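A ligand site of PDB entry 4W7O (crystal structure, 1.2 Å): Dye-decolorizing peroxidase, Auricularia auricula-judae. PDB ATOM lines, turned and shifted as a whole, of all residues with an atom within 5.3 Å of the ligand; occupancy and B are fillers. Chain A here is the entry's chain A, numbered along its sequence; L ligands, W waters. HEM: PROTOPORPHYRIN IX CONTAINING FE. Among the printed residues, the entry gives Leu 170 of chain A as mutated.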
ATOM      1  N   GLU A 163      -8.378 -20.673  28.612  1.00  0.00           N
ATOM      2  CA  GLU A 163      -7.190 -21.079  27.904  1.00  0.00           C
ATOM      3  C   GLU A 163      -6.007 -21.111  28.879  1.00  0.00           C
ATOM      4  O   GLU A 163      -6.155 -20.777  30.061  1.00  0.00           O
ATOM      5  CB  GLU A 163      -6.988 -20.252  26.622  1.00  0.00           C
ATOM      6  CG  GLU A 163      -6.986 -18.768  26.821  1.00  0.00           C
ATOM      7  CD  GLU A 163      -5.783 -18.322  27.606  1.00  0.00           C
ATOM      8  OE1 GLU A 163      -5.947 -17.619  28.616  1.00  0.00           O
ATOM      9  OE2 GLU A 163      -4.653 -18.685  27.217  1.00  0.00           O
ATOM     10  N   PHE A 165      -3.334 -19.356  29.571  1.00  0.00           N
ATOM     11  CA  PHE A 165      -2.939 -18.170  30.335  1.00  0.00           C
ATOM     12  C   PHE A 165      -3.934 -17.856  31.450  1.00  0.00           C
ATOM     13  O   PHE A 165      -3.654 -16.996  32.283  1.00  0.00           O
ATOM     14  CB  PHE A 165      -2.825 -16.921  29.452  1.00  0.00           C
ATOM     15  CG  PHE A 165      -1.665 -16.919  28.485  1.00  0.00           C
ATOM     16  CD1 PHE A 165      -0.411 -17.419  28.808  1.00  0.00           C
ATOM     17  CD2 PHE A 165      -1.841 -16.376  27.229  1.00  0.00           C
ATOM     18  CE1 PHE A 165       0.630 -17.369  27.896  1.00  0.00           C
ATOM     19  CE2 PHE A 165      -0.808 -16.333  26.306  1.00  0.00           C
ATOM     20  CZ  PHE A 165       0.416 -16.843  26.638  1.00  0.00           C
ATOM     21  N   PHE A 167      -7.462 -17.161  30.900  1.00  0.00           N
ATOM     22  CA  PHE A 167      -8.608 -16.327  30.517  1.00  0.00           C
ATOM     23  C   PHE A 167      -9.758 -17.149  29.980  1.00  0.00           C
ATOM     24  O   PHE A 167      -9.551 -18.052  29.160  1.00  0.00           O
ATOM     25  CB  PHE A 167      -8.201 -15.285  29.460  1.00  0.00           C
ATOM     26  CG  PHE A 167      -7.197 -14.271  29.966  1.00  0.00           C
ATOM     27  CD1 PHE A 167      -5.849 -14.611  30.117  1.00  0.00           C
ATOM     28  CD2 PHE A 167      -7.594 -12.995  30.323  1.00  0.00           C
ATOM     29  CE1 PHE A 167      -4.941 -13.675  30.634  1.00  0.00           C
ATOM     30  CE2 PHE A 167      -6.692 -12.061  30.817  1.00  0.00           C
ATOM     31  CZ  PHE A 167      -5.365 -12.401  30.973  1.00  0.00           C
ATOM     32  N   LEU A 168     -10.974 -16.824  30.416  1.00  0.00           N
ATOM     33  CA  LEU A 168     -12.154 -17.449  29.831  1.00  0.00           C
ATOM     34  C   LEU A 168     -12.174 -17.214  28.328  1.00  0.00           C
ATOM     35  O   LEU A 168     -12.009 -16.089  27.865  1.00  0.00           O
ATOM     36  CB  LEU A 168     -13.413 -16.886  30.497  1.00  0.00           C
ATOM     37  CG  LEU A 168     -14.725 -17.529  30.049  1.00  0.00           C
ATOM     38  CD1 LEU A 168     -14.763 -19.045  30.341  1.00  0.00           C
ATOM     39  CD2 LEU A 168     -15.894 -16.815  30.710  1.00  0.00           C
ATOM     40  N   ASP A 169     -12.334 -18.288  27.568  1.00  0.00           N
ATOM     41  CA  ASP A 169     -12.257 -18.227  26.119  1.00  0.00           C
ATOM     42  C   ASP A 169     -13.591 -18.617  25.470  1.00  0.00           C
ATOM     43  O   ASP A 169     -14.495 -19.154  26.110  1.00  0.00           O
ATOM     44  CB  ASP A 169     -11.157 -19.172  25.649  1.00  0.00           C
ATOM     45  CG  ASP A 169     -10.694 -18.922  24.213  1.00  0.00           C
ATOM     46  OD1 ASP A 169     -10.961 -17.827  23.647  1.00  0.00           O
ATOM     47  OD2 ASP A 169     -10.036 -19.841  23.670  1.00  0.00           O
ATOM     48  N   LEU A 170     -13.675 -18.328  24.185  1.00  0.00           N
ATOM     49  CA  LEU A 170     -14.819 -18.668  23.347  1.00  0.00           C
ATOM     50  C   LEU A 170     -16.101 -17.989  23.816  1.00  0.00           C
ATOM     51  O   LEU A 170     -17.183 -18.523  23.653  1.00  0.00           O
ATOM     52  CB  LEU A 170     -14.987 -20.201  23.191  1.00  0.00           C
ATOM     53  CG  LEU A 170     -13.732 -20.899  22.655  1.00  0.00           C
ATOM     54  CD1 LEU A 170     -14.005 -22.383  22.444  1.00  0.00           C
ATOM     55  CD2 LEU A 170     -13.206 -20.290  21.362  1.00  0.00           C
ATOM     56  N   ILE A 171     -15.955 -16.793  24.358  1.00  0.00           N
ATOM     57  CA  ILE A 171     -17.082 -15.948  24.714  1.00  0.00           C
ATOM     58  C   ILE A 171     -17.716 -15.351  23.465  1.00  0.00           C
ATOM     59  O   ILE A 171     -18.934 -15.365  23.296  1.00  0.00           O
ATOM     60  CB  ILE A 171     -16.631 -14.800  25.650  1.00  0.00           C
ATOM     61  CG1 ILE A 171     -16.113 -15.385  26.964  1.00  0.00           C
ATOM     62  CG2 ILE A 171     -17.753 -13.811  25.878  1.00  0.00           C
ATOM     63  CD1 ILE A 171     -15.412 -14.382  27.845  1.00  0.00           C
ATOM     64  N   ALA A 172     -16.861 -14.805  22.608  1.00  0.00           N
ATOM     65  CA  ALA A 172     -17.318 -13.952  21.528  1.00  0.00           C
ATOM     66  C   ALA A 172     -17.212 -14.661  20.178  1.00  0.00           C
ATOM     67  O   ALA A 172     -16.118 -15.036  19.774  1.00  0.00           O
ATOM     68  CB  ALA A 172     -16.499 -12.668  21.526  1.00  0.00           C
ATOM     69  N   GLN A 173     -18.320 -14.807  19.483  1.00  0.00           N
ATOM     70  CA  GLN A 173     -18.407 -15.443  18.165  1.00  0.00           C
ATOM     71  C   GLN A 173     -19.347 -14.618  17.333  1.00  0.00           C
ATOM     72  O   GLN A 173     -20.261 -13.988  17.875  1.00  0.00           O
ATOM     73  CB  GLN A 173     -18.992 -16.861  18.284  1.00  0.00           C
ATOM     74  CG  GLN A 173     -18.289 -17.794  19.269  1.00  0.00           C
ATOM     75  CD  GLN A 173     -17.098 -18.521  18.680  1.00  0.00           C
ATOM     76  OE1 GLN A 173     -16.471 -18.087  17.716  1.00  0.00           O
ATOM     77  NE2 GLN A 173     -16.781 -19.655  19.285  1.00  0.00           N
ATOM     78  N   LEU A 220      -0.328 -23.529  18.704  1.00  0.00           N
ATOM     79  CA  LEU A 220       0.229 -22.330  19.303  1.00  0.00           C
ATOM     80  C   LEU A 220       0.678 -22.602  20.719  1.00  0.00           C
ATOM     81  O   LEU A 220      -0.134 -22.692  21.649  1.00  0.00           O
ATOM     82  CB  LEU A 220      -0.809 -21.208  19.246  1.00  0.00           C
ATOM     83  CG  LEU A 220      -1.258 -20.812  17.837  1.00  0.00           C
ATOM     84  CD1 LEU A 220      -2.291 -19.705  17.895  1.00  0.00           C
ATOM     85  CD2 LEU A 220      -0.098 -20.422  16.942  1.00  0.00           C
ATOM     86  N   GLN A 222       2.080 -21.820  24.331  1.00  0.00           N
ATOM     87  CA  GLN A 222       1.986 -20.695  25.250  1.00  0.00           C
ATOM     88  C   GLN A 222       3.003 -20.843  26.382  1.00  0.00           C
ATOM     89  O   GLN A 222       3.107 -21.899  27.010  1.00  0.00           O
ATOM     90  CB  GLN A 222       0.577 -20.603  25.820  1.00  0.00           C
ATOM     91  CG  GLN A 222      -0.424 -20.219  24.768  1.00  0.00           C
ATOM     92  CD  GLN A 222      -1.834 -20.300  25.257  1.00  0.00           C
ATOM     93  OE1 GLN A 222      -2.547 -21.231  24.930  1.00  0.00           O
ATOM     94  NE2 GLN A 222      -2.252 -19.326  26.055  1.00  0.00           N
ATOM     95  N   VAL A 254      -5.212  -8.522  26.802  1.00  0.00           N
ATOM     96  CA  VAL A 254      -6.218  -9.374  26.181  1.00  0.00           C
ATOM     97  C   VAL A 254      -7.433  -8.563  25.725  1.00  0.00           C
ATOM     98  O   VAL A 254      -8.010  -8.817  24.658  1.00  0.00           O
ATOM     99  CB  VAL A 254      -6.666 -10.512  27.153  1.00  0.00           C
ATOM    100  CG1 VAL A 254      -7.848 -11.299  26.616  1.00  0.00           C
ATOM    101  CG2 VAL A 254      -5.500 -11.457  27.446  1.00  0.00           C
ATOM    102  N   ARG A 256      -9.931  -8.446  28.003  1.00  0.00           N
ATOM    103  CA  ARG A 256     -10.856  -8.965  29.002  1.00  0.00           C
ATOM    104  C   ARG A 256     -10.047  -9.369  30.214  1.00  0.00           C
ATOM    105  O   ARG A 256      -8.893  -9.757  30.072  1.00  0.00           O
ATOM    106  CB  ARG A 256     -11.609 -10.198  28.507  1.00  0.00           C
ATOM    107  CG  ARG A 256     -12.486  -9.990  27.304  1.00  0.00           C
ATOM    108  CD  ARG A 256     -13.299 -11.264  26.998  1.00  0.00           C
ATOM    109  NE  ARG A 256     -14.185 -11.036  25.867  1.00  0.00           N
ATOM    110  CZ  ARG A 256     -15.404 -10.514  25.939  1.00  0.00           C
ATOM    111  NH1 ARG A 256     -15.938 -10.245  27.116  1.00  0.00           N
ATOM    112  NH2 ARG A 256     -16.059 -10.260  24.823  1.00  0.00           N
ATOM    113  N   ASN A 282     -20.581  -8.941  26.290  1.00  0.00           N
ATOM    114  CA  ASN A 282     -20.173  -8.574  24.935  1.00  0.00           C
ATOM    115  C   ASN A 282     -20.793  -7.274  24.468  1.00  0.00           C
ATOM    116  O   ASN A 282     -20.610  -6.885  23.320  1.00  0.00           O
ATOM    117  CB  ASN A 282     -20.460  -9.698  23.933  1.00  0.00           C
ATOM    118  CG  ASN A 282     -19.365  -9.810  22.881  1.00  0.00           C
ATOM    119  OD1 ASN A 282     -18.258  -9.287  23.073  1.00  0.00           O
ATOM    120  ND2 ASN A 282     -19.652 -10.459  21.777  1.00  0.00           N
ATOM    121  N   TYR A 286     -16.445  -0.198  21.919  1.00  0.00           N
ATOM    122  CA  TYR A 286     -15.234   0.617  22.150  1.00  0.00           C
ATOM    123  C   TYR A 286     -15.481   2.122  22.159  1.00  0.00           C
ATOM    124  O   TYR A 286     -14.607   2.883  22.540  1.00  0.00           O
ATOM    125  CB  TYR A 286     -14.050   0.253  21.239  1.00  0.00           C
ATOM    126  CG  TYR A 286     -13.613  -1.180  21.410  1.00  0.00           C
ATOM    127  CD1 TYR A 286     -13.215  -1.674  22.643  1.00  0.00           C
ATOM    128  CD2 TYR A 286     -13.601  -2.056  20.327  1.00  0.00           C
ATOM    129  CE1 TYR A 286     -12.849  -2.990  22.798  1.00  0.00           C
ATOM    130  CE2 TYR A 286     -13.229  -3.383  20.486  1.00  0.00           C
ATOM    131  CZ  TYR A 286     -12.847  -3.835  21.723  1.00  0.00           C
ATOM    132  OH  TYR A 286     -12.482  -5.134  21.927  1.00  0.00           O
ATOM    133  N   HIS A 305      -5.795  -7.626  22.356  1.00  0.00           N
ATOM    134  CA  HIS A 305      -6.051  -8.742  21.457  1.00  0.00           C
ATOM    135  C   HIS A 305      -7.451  -8.709  20.854  1.00  0.00           C
ATOM    136  O   HIS A 305      -7.590  -8.837  19.645  1.00  0.00           O
ATOM    137  CB  HIS A 305      -5.762 -10.048  22.185  1.00  0.00           C
ATOM    138  CG  HIS A 305      -6.089 -11.281  21.384  1.00  0.00           C
ATOM    139  ND1 HIS A 305      -5.528 -11.535  20.148  1.00  0.00           N
ATOM    140  CD2 HIS A 305      -6.910 -12.322  21.652  1.00  0.00           C
ATOM    141  CE1 HIS A 305      -5.984 -12.700  19.711  1.00  0.00           C
ATOM    142  NE2 HIS A 305      -6.827 -13.191  20.592  1.00  0.00           N
ATOM    143  N   ILE A 306      -8.491  -8.563  21.676  1.00  0.00           N
ATOM    144  CA  ILE A 306      -9.837  -8.653  21.116  1.00  0.00           C
ATOM    145  C   ILE A 306     -10.166  -7.445  20.273  1.00  0.00           C
ATOM    146  O   ILE A 306     -10.977  -7.550  19.346  1.00  0.00           O
ATOM    147  CB  ILE A 306     -10.922  -8.926  22.187  1.00  0.00           C
ATOM    148  CG1 ILE A 306     -11.050  -7.798  23.208  1.00  0.00           C
ATOM    149  CG2 ILE A 306     -10.683 -10.280  22.815  1.00  0.00           C
ATOM    150  CD1 ILE A 306     -12.386  -7.851  23.920  1.00  0.00           C
ATOM    151  N   THR A 309      -8.677  -8.195  16.935  1.00  0.00           N
ATOM    152  CA  THR A 309      -9.321  -9.262  16.174  1.00  0.00           C
ATOM    153  C   THR A 309     -10.779  -9.021  15.872  1.00  0.00           C
ATOM    154  O   THR A 309     -11.300  -9.620  14.952  1.00  0.00           O
ATOM    155  CB  THR A 309      -9.126 -10.618  16.826  1.00  0.00           C
ATOM    156  OG1 THR A 309      -9.732 -10.595  18.108  1.00  0.00           O
ATOM    157  CG2 THR A 309      -7.673 -11.005  16.921  1.00  0.00           C
ATOM    158  N   ARG A 310     -11.429  -8.117  16.597  1.00  0.00           N
ATOM    159  CA  ARG A 310     -12.755  -7.593  16.222  1.00  0.00           C
ATOM    160  C   ARG A 310     -12.791  -6.112  16.579  1.00  0.00           C
ATOM    161  O   ARG A 310     -13.067  -5.739  17.708  1.00  0.00           O
ATOM    162  CB  ARG A 310     -13.922  -8.347  16.867  1.00  0.00           C
ATOM    163  CG  ARG A 310     -15.242  -7.784  16.363  1.00  0.00           C
ATOM    164  CD  ARG A 310     -16.470  -8.283  17.123  1.00  0.00           C
ATOM    165  NE  ARG A 310     -17.649  -7.509  16.704  1.00  0.00           N
ATOM    166  CZ  ARG A 310     -18.747  -7.352  17.442  1.00  0.00           C
ATOM    167  NH1 ARG A 310     -18.899  -8.014  18.579  1.00  0.00           N
ATOM    168  NH2 ARG A 310     -19.717  -6.558  17.027  1.00  0.00           N
ATOM    169  N   ARG A 312     -14.692  -3.601  15.984  1.00  0.00           N
ATOM    170  CA  ARG A 312     -15.960  -2.957  16.288  1.00  0.00           C
ATOM    171  C   ARG A 312     -15.939  -1.517  15.772  1.00  0.00           C
ATOM    172  O   ARG A 312     -15.676  -1.306  14.593  1.00  0.00           O
ATOM    173  CB  ARG A 312     -16.310  -3.066  17.778  1.00  0.00           C
ATOM    174  CG  ARG A 312     -16.265  -4.513  18.262  1.00  0.00           C
ATOM    175  CD  ARG A 312     -16.719  -4.688  19.692  1.00  0.00           C
ATOM    176  NE  ARG A 312     -16.375  -6.025  20.164  1.00  0.00           N
ATOM    177  CZ  ARG A 312     -17.089  -6.782  20.979  1.00  0.00           C
ATOM    178  NH1 ARG A 312     -18.256  -6.385  21.471  1.00  0.00           N
ATOM    179  NH2 ARG A 312     -16.646  -7.997  21.260  1.00  0.00           N
ATOM    180  N   ILE A 331     -14.581 -14.863  12.238  1.00  0.00           N
ATOM    181  CA  ILE A 331     -14.247 -16.275  12.273  1.00  0.00           C
ATOM    182  C   ILE A 331     -15.047 -16.945  13.379  1.00  0.00           C
ATOM    183  O   ILE A 331     -15.329 -16.319  14.406  1.00  0.00           O
ATOM    184  CB  ILE A 331     -12.727 -16.517  12.491  1.00  0.00           C
ATOM    185  CG1 ILE A 331     -12.213 -15.882  13.807  1.00  0.00           C
ATOM    186  CG2 ILE A 331     -11.927 -16.007  11.292  1.00  0.00           C
ATOM    187  CD1 ILE A 331     -10.796 -16.321  14.150  1.00  0.00           C
ATOM    188  N   ARG A 333     -14.608 -19.754  16.201  1.00  0.00           N
ATOM    189  CA  ARG A 333     -13.478 -20.385  16.888  1.00  0.00           C
ATOM    190  C   ARG A 333     -13.891 -21.624  17.664  1.00  0.00           C
ATOM    191  O   ARG A 333     -14.877 -21.610  18.386  1.00  0.00           O
ATOM    192  CB  ARG A 333     -12.795 -19.392  17.808  1.00  0.00           C
ATOM    193  CG  ARG A 333     -12.065 -18.280  17.064  1.00  0.00           C
ATOM    194  CD  ARG A 333     -11.448 -17.241  17.991  1.00  0.00           C
ATOM    195  NE  ARG A 333     -12.529 -16.626  18.772  1.00  0.00           N
ATOM    196  CZ  ARG A 333     -12.569 -16.504  20.094  1.00  0.00           C
ATOM    197  NH1 ARG A 333     -11.549 -16.889  20.836  1.00  0.00           N
ATOM    198  NH2 ARG A 333     -13.641 -15.982  20.663  1.00  0.00           N
ATOM    199  N   LEU A 358      -2.509 -23.716  22.850  1.00  0.00           N
ATOM    200  CA  LEU A 358      -3.830 -23.729  22.271  1.00  0.00           C
ATOM    201  C   LEU A 358      -3.790 -24.445  20.934  1.00  0.00           C
ATOM    202  O   LEU A 358      -2.989 -24.112  20.068  1.00  0.00           O
ATOM    203  CB  LEU A 358      -4.301 -22.295  22.074  1.00  0.00           C
ATOM    204  CG  LEU A 358      -5.725 -22.125  21.547  1.00  0.00           C
ATOM    205  CD1 LEU A 358      -6.738 -22.661  22.561  1.00  0.00           C
ATOM    206  CD2 LEU A 358      -6.005 -20.667  21.206  1.00  0.00           C
ATOM    207  N   PHE A 360      -5.513 -24.161  18.128  1.00  0.00           N
ATOM    208  CA  PHE A 360      -6.353 -23.115  17.601  1.00  0.00           C
ATOM    209  C   PHE A 360      -7.039 -23.603  16.342  1.00  0.00           C
ATOM    210  O   PHE A 360      -6.398 -24.139  15.452  1.00  0.00           O
ATOM    211  CB  PHE A 360      -5.515 -21.874  17.328  1.00  0.00           C
ATOM    212  CG  PHE A 360      -6.258 -20.773  16.627  1.00  0.00           C
ATOM    213  CD1 PHE A 360      -6.285 -20.705  15.259  1.00  0.00           C
ATOM    214  CD2 PHE A 360      -6.900 -19.798  17.359  1.00  0.00           C
ATOM    215  CE1 PHE A 360      -6.965 -19.693  14.619  1.00  0.00           C
ATOM    216  CE2 PHE A 360      -7.596 -18.797  16.729  1.00  0.00           C
ATOM    217  CZ  PHE A 360      -7.616 -18.738  15.351  1.00  0.00           C
ATOM    218  N   PHE A 371      -8.923 -15.845   9.236  1.00  0.00           N
ATOM    219  CA  PHE A 371      -7.665 -16.047   9.953  1.00  0.00           C
ATOM    220  C   PHE A 371      -6.479 -15.286   9.349  1.00  0.00           C
ATOM    221  O   PHE A 371      -5.748 -14.593  10.065  1.00  0.00           O
ATOM    222  CB  PHE A 371      -7.331 -17.535  10.068  1.00  0.00           C
ATOM    223  CG  PHE A 371      -5.915 -17.770  10.464  1.00  0.00           C
ATOM    224  CD1 PHE A 371      -5.503 -17.522  11.773  1.00  0.00           C
ATOM    225  CD2 PHE A 371      -4.973 -18.144   9.527  1.00  0.00           C
ATOM    226  CE1 PHE A 371      -4.173 -17.671  12.126  1.00  0.00           C
ATOM    227  CE2 PHE A 371      -3.644 -18.303   9.877  1.00  0.00           C
ATOM    228  CZ  PHE A 371      -3.247 -18.062  11.182  1.00  0.00           C
ATOM    229  N   LEU A 374      -6.761 -11.514   9.958  1.00  0.00           N
ATOM    230  CA  LEU A 374      -6.635 -11.103  11.346  1.00  0.00           C
ATOM    231  C   LEU A 374      -5.199 -11.202  11.807  1.00  0.00           C
ATOM    232  O   LEU A 374      -4.717 -10.360  12.566  1.00  0.00           O
ATOM    233  CB  LEU A 374      -7.577 -11.949  12.216  1.00  0.00           C
ATOM    234  CG  LEU A 374      -9.054 -11.749  11.915  1.00  0.00           C
ATOM    235  CD1 LEU A 374      -9.888 -12.736  12.731  1.00  0.00           C
ATOM    236  CD2 LEU A 374      -9.520 -10.332  12.180  1.00  0.00           C
ATOM    237  N   GLN A 375      -4.473 -12.220  11.360  1.00  0.00           N
ATOM    238  CA  GLN A 375      -3.078 -12.351  11.733  1.00  0.00           C
ATOM    239  C   GLN A 375      -2.186 -11.294  11.048  1.00  0.00           C
ATOM    240  O   GLN A 375      -1.377 -10.634  11.710  1.00  0.00           O
ATOM    241  CB  GLN A 375      -2.567 -13.774  11.441  1.00  0.00           C
ATOM    242  CG  GLN A 375      -1.149 -14.040  11.976  1.00  0.00           C
ATOM    243  CD  GLN A 375      -1.130 -14.166  13.467  1.00  0.00           C
ATOM    244  OE1 GLN A 375      -1.874 -14.949  14.034  1.00  0.00           O
ATOM    245  NE2 GLN A 375      -0.276 -13.374  14.129  1.00  0.00           N
ATOM    246  N   ILE A 398      -0.686 -10.614  22.422  1.00  0.00           N
ATOM    247  CA  ILE A 398      -0.912 -12.054  22.563  1.00  0.00           C
ATOM    248  C   ILE A 398      -0.393 -12.817  21.356  1.00  0.00           C
ATOM    249  O   ILE A 398       0.383 -13.762  21.506  1.00  0.00           O
ATOM    250  CB  ILE A 398      -2.401 -12.345  22.869  1.00  0.00           C
ATOM    251  CG1 ILE A 398      -2.866 -11.542  24.101  1.00  0.00           C
ATOM    252  CG2 ILE A 398      -2.602 -13.855  23.058  1.00  0.00           C
ATOM    253  CD1 ILE A 398      -2.055 -11.777  25.379  1.00  0.00           C
ATOM    254  N   ILE A 399      -0.797 -12.418  20.160  1.00  0.00           N
ATOM    255  CA  ILE A 399      -0.495 -13.201  18.955  1.00  0.00           C
ATOM    256  C   ILE A 399       0.343 -12.479  17.905  1.00  0.00           C
ATOM    257  O   ILE A 399       0.691 -13.077  16.901  1.00  0.00           O
ATOM    258  CB  ILE A 399      -1.773 -13.743  18.267  1.00  0.00           C
ATOM    259  CG1 ILE A 399      -2.689 -12.589  17.794  1.00  0.00           C
ATOM    260  CG2 ILE A 399      -2.519 -14.716  19.177  1.00  0.00           C
ATOM    261  CD1 ILE A 399      -3.738 -13.008  16.772  1.00  0.00           C
ATOM    262  N   VAL A 427       3.452 -16.506  22.814  1.00  0.00           N
ATOM    263  CA  VAL A 427       2.799 -17.497  21.979  1.00  0.00           C
ATOM    264  C   VAL A 427       3.754 -17.802  20.848  1.00  0.00           C
ATOM    265  O   VAL A 427       4.215 -16.902  20.132  1.00  0.00           O
ATOM    266  CB  VAL A 427       1.452 -17.002  21.430  1.00  0.00           C
ATOM    267  CG1 VAL A 427       0.859 -18.009  20.426  1.00  0.00           C
ATOM    268  CG2 VAL A 427       0.469 -16.742  22.582  1.00  0.00           C
HETATM  269  CHA HEM L   1     -10.771 -13.700  21.629  1.00  0.00           C
HETATM  270  CHB HEM L   1      -6.975 -15.898  23.653  1.00  0.00           C
HETATM  271  CHC HEM L   1      -5.214 -16.905  19.250  1.00  0.00           C
HETATM  272  CHD HEM L   1      -8.846 -14.463  17.233  1.00  0.00           C
HETATM  273  C1A HEM L   1      -9.914 -14.212  22.561  1.00  0.00           C
HETATM  274  C2A HEM L   1     -10.051 -14.126  23.997  1.00  0.00           C
HETATM  275  C3A HEM L   1      -9.012 -14.747  24.544  1.00  0.00           C
HETATM  276  C4A HEM L   1      -8.160 -15.220  23.479  1.00  0.00           C
HETATM  277  CMA HEM L   1      -8.718 -14.964  26.036  1.00  0.00           C
HETATM  278  CAA HEM L   1     -11.217 -13.461  24.747  1.00  0.00           C
HETATM  279  CBA HEM L   1     -12.408 -14.409  24.835  1.00  0.00           C
HETATM  280  CGA HEM L   1     -13.460 -14.094  23.787  1.00  0.00           C
HETATM  281  O1A HEM L   1     -13.664 -12.883  23.573  1.00  0.00           O
HETATM  282  O2A HEM L   1     -14.103 -15.018  23.277  1.00  0.00           O
HETATM  283  C1B HEM L   1      -6.147 -16.358  22.657  1.00  0.00           C
HETATM  284  C2B HEM L   1      -4.910 -17.072  22.825  1.00  0.00           C
HETATM  285  C3B HEM L   1      -4.421 -17.330  21.596  1.00  0.00           C
HETATM  286  C4B HEM L   1      -5.356 -16.838  20.612  1.00  0.00           C
HETATM  287  CMB HEM L   1      -4.269 -17.372  24.200  1.00  0.00           C
HETATM  288  CAB HEM L   1      -3.140 -18.082  21.224  1.00  0.00           C
HETATM  289  CBB HEM L   1      -2.588 -19.026  21.990  1.00  0.00           C
HETATM  290  C1C HEM L   1      -6.000 -16.268  18.332  1.00  0.00           C
HETATM  291  C2C HEM L   1      -5.720 -16.164  16.915  1.00  0.00           C
HETATM  292  C3C HEM L   1      -6.700 -15.472  16.358  1.00  0.00           C
HETATM  293  C4C HEM L   1      -7.652 -15.131  17.404  1.00  0.00           C
HETATM  294  CMC HEM L   1      -4.498 -16.804  16.237  1.00  0.00           C
HETATM  295  CAC HEM L   1      -6.877 -15.037  14.906  1.00  0.00           C
HETATM  296  CBC HEM L   1      -5.883 -14.886  14.020  1.00  0.00           C
HETATM  297  C1D HEM L   1      -9.751 -14.120  18.224  1.00  0.00           C
HETATM  298  C2D HEM L   1     -11.034 -13.525  17.978  1.00  0.00           C
HETATM  299  C3D HEM L   1     -11.608 -13.268  19.310  1.00  0.00           C
HETATM  300  C4D HEM L   1     -10.649 -13.753  20.261  1.00  0.00           C
HETATM  301  CMD HEM L   1     -11.728 -13.223  16.650  1.00  0.00           C
HETATM  302  CAD HEM L   1     -12.963 -12.647  19.584  1.00  0.00           C
HETATM  303  CBD HEM L   1     -12.937 -11.135  19.341  1.00  0.00           C
HETATM  304  CGD HEM L   1     -14.288 -10.499  19.464  1.00  0.00           C
HETATM  305  O1D HEM L   1     -14.424  -9.512  20.227  1.00  0.00           O
HETATM  306  O2D HEM L   1     -15.240 -10.987  18.802  1.00  0.00           O
HETATM  307  NA  HEM L   1      -8.749 -14.866  22.289  1.00  0.00           N
HETATM  308  NB  HEM L   1      -6.378 -16.253  21.301  1.00  0.00           N
HETATM  309  NC  HEM L   1      -7.179 -15.603  18.607  1.00  0.00           N
HETATM  310  ND  HEM L   1      -9.548 -14.267  19.587  1.00  0.00           N
HETATM  311 FE   HEM L   1      -7.854 -15.039  20.443  1.00  0.00          FE
HETATM  312  O   HOH W   1     -13.661  -6.850  20.142  1.00  0.00           O
HETATM  313  O   HOH W   2      -8.992 -18.363  21.265  1.00  0.00           O
HETATM  314  O   HOH W   3     -15.657 -12.962  16.992  1.00  0.00           O
HETATM  315  O   HOH W   4     -17.802 -10.434  19.417  1.00  0.00           O
HETATM  316  O   HOH W   5     -14.227 -10.532  22.752  1.00  0.00           O
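A ring nitrogen (NE2) of His 305 is bound to an iron atom (FE) of the ligand (2.1 Å). An oxygen (O2A) of the ligand sits at hydrogen-bond distance from the backbone NH of Ile 171 (2.8 Å). NH2 of Arg 333 is in salt-bridge range of O2A of the ligand. O2A of the ligand lies within hydrogen-bond range of N of Leu 170, 3.5 Å away. An oxygen (O1D) of the ligand is in salt-bridge range of the guanidinium group of Arg 312 (2.9 Å). The guanidinium group (NE) of Arg 256 lies within salt-bridge range of an oxygen (O1A) of the ligand (3.0 Å). The backbone NH (N) of Ala 172 is in hydrogen-bond range of an oxygen (O2A) of the ligand, at 2.8 Å.
The side-chain carboxylate (OE2) of Glu 163 is in hydrogen-bond range of the backbone NH (N) of Phe 165 (2.8 Å). NH2 of Arg 312 sits at hydrogen-bond distance from OD1 of Asn 282 (2.7 Å). The guanidinium group (NH2) of Arg 256 sits at hydrogen-bond distance from the side-chain amide oxygen (OD1) of Asn 282 (3.0 Å). O of Leu 220 lies within hydrogen-bond range of N of Leu 358 (2.9 Å). The backbone carbonyl oxygen (O) of Ala 172 is in hydrogen-bond range of the guanidinium group (NH2) of Arg 333 (2.8 Å). The backbone NH (N) of His 305 lies within hydrogen-bond range of the backbone carbonyl oxygen (O) of Val 254 (3.4 Å). The side-chain amide nitrogen (NE2) of Gln 222 sits at hydrogen-bond distance from the side-chain carboxylate (OE2) of Glu 163 (2.7 Å). The backbone NH (N) of Leu 358 lies within hydrogen-bond range of the side-chain amide oxygen (OE1) of Gln 222, at 3.2 Å.
Glu 163 touches the ligand. Phe 167 touches the ligand (CB to CMA, 3.5 Å). O of Leu 168 touches CBA of the ligand, 3.5 Å away. Asp 169 touches the ligand. Leu 220 touches the ligand (CD1 to CAB, 3.8 Å). NE2 of Gln 222 touches CMB of the ligand, at 3.4 Å. Val 254 touches the ligand (CG1 to CMA, 3.8 Å). Ile 306 touches the ligand. OG1 of Thr 309 touches C2D of the ligand (3.2 Å). Arg 310 touches the ligand. Ile 331 touches the ligand (CG1 to CMD, 3.9 Å). Leu 358 touches the ligand. Phe 360 touches the ligand (CE2 to C2C, 3.2 Å). Phe 371 touches the ligand. Leu 374 touches the ligand. Gln 375 touches the ligand (OE1 to CMC, 3.9 Å). Ile 398 touches the ligand. Ile 399 touches the ligand (CG2 to CHC, 3.5 Å). Val 427 touches the ligand (CG2 to CBB, 3.9 Å). Within 4 Å of the ligand: Glu 163, Phe 167, Leu 168, Asp 169, Leu 170, Ile 171, Ala 172, Leu 220, Gln 222, Val 254, Arg 256, His 305, Ile 306, Thr 309, Arg 310, Arg 312, Ile 331, Arg 333, Leu 358, Phe 360, Phe 371, Leu 374, Gln 375, Ile 398, Ile 399 and Val 427. The nearest printed residue that does not touch the ligand is Phe 165 (4.01 Å).
Water W5 bridges O1A of the ligand and NH2 of Arg 256. Water W1 lies within hydrogen-bond range of O of Arg 310 (2.7 Å), OH of Tyr 286 (2.7 Å), O1D of the ligand (2.8 Å), NE of Arg 312 (2.8 Å) and O of Ile 306 (2.9 Å). Water W2 bridges NH1 of Arg 333 (3.0 Å) and OD2 of Asp 169 (3.0 Å).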
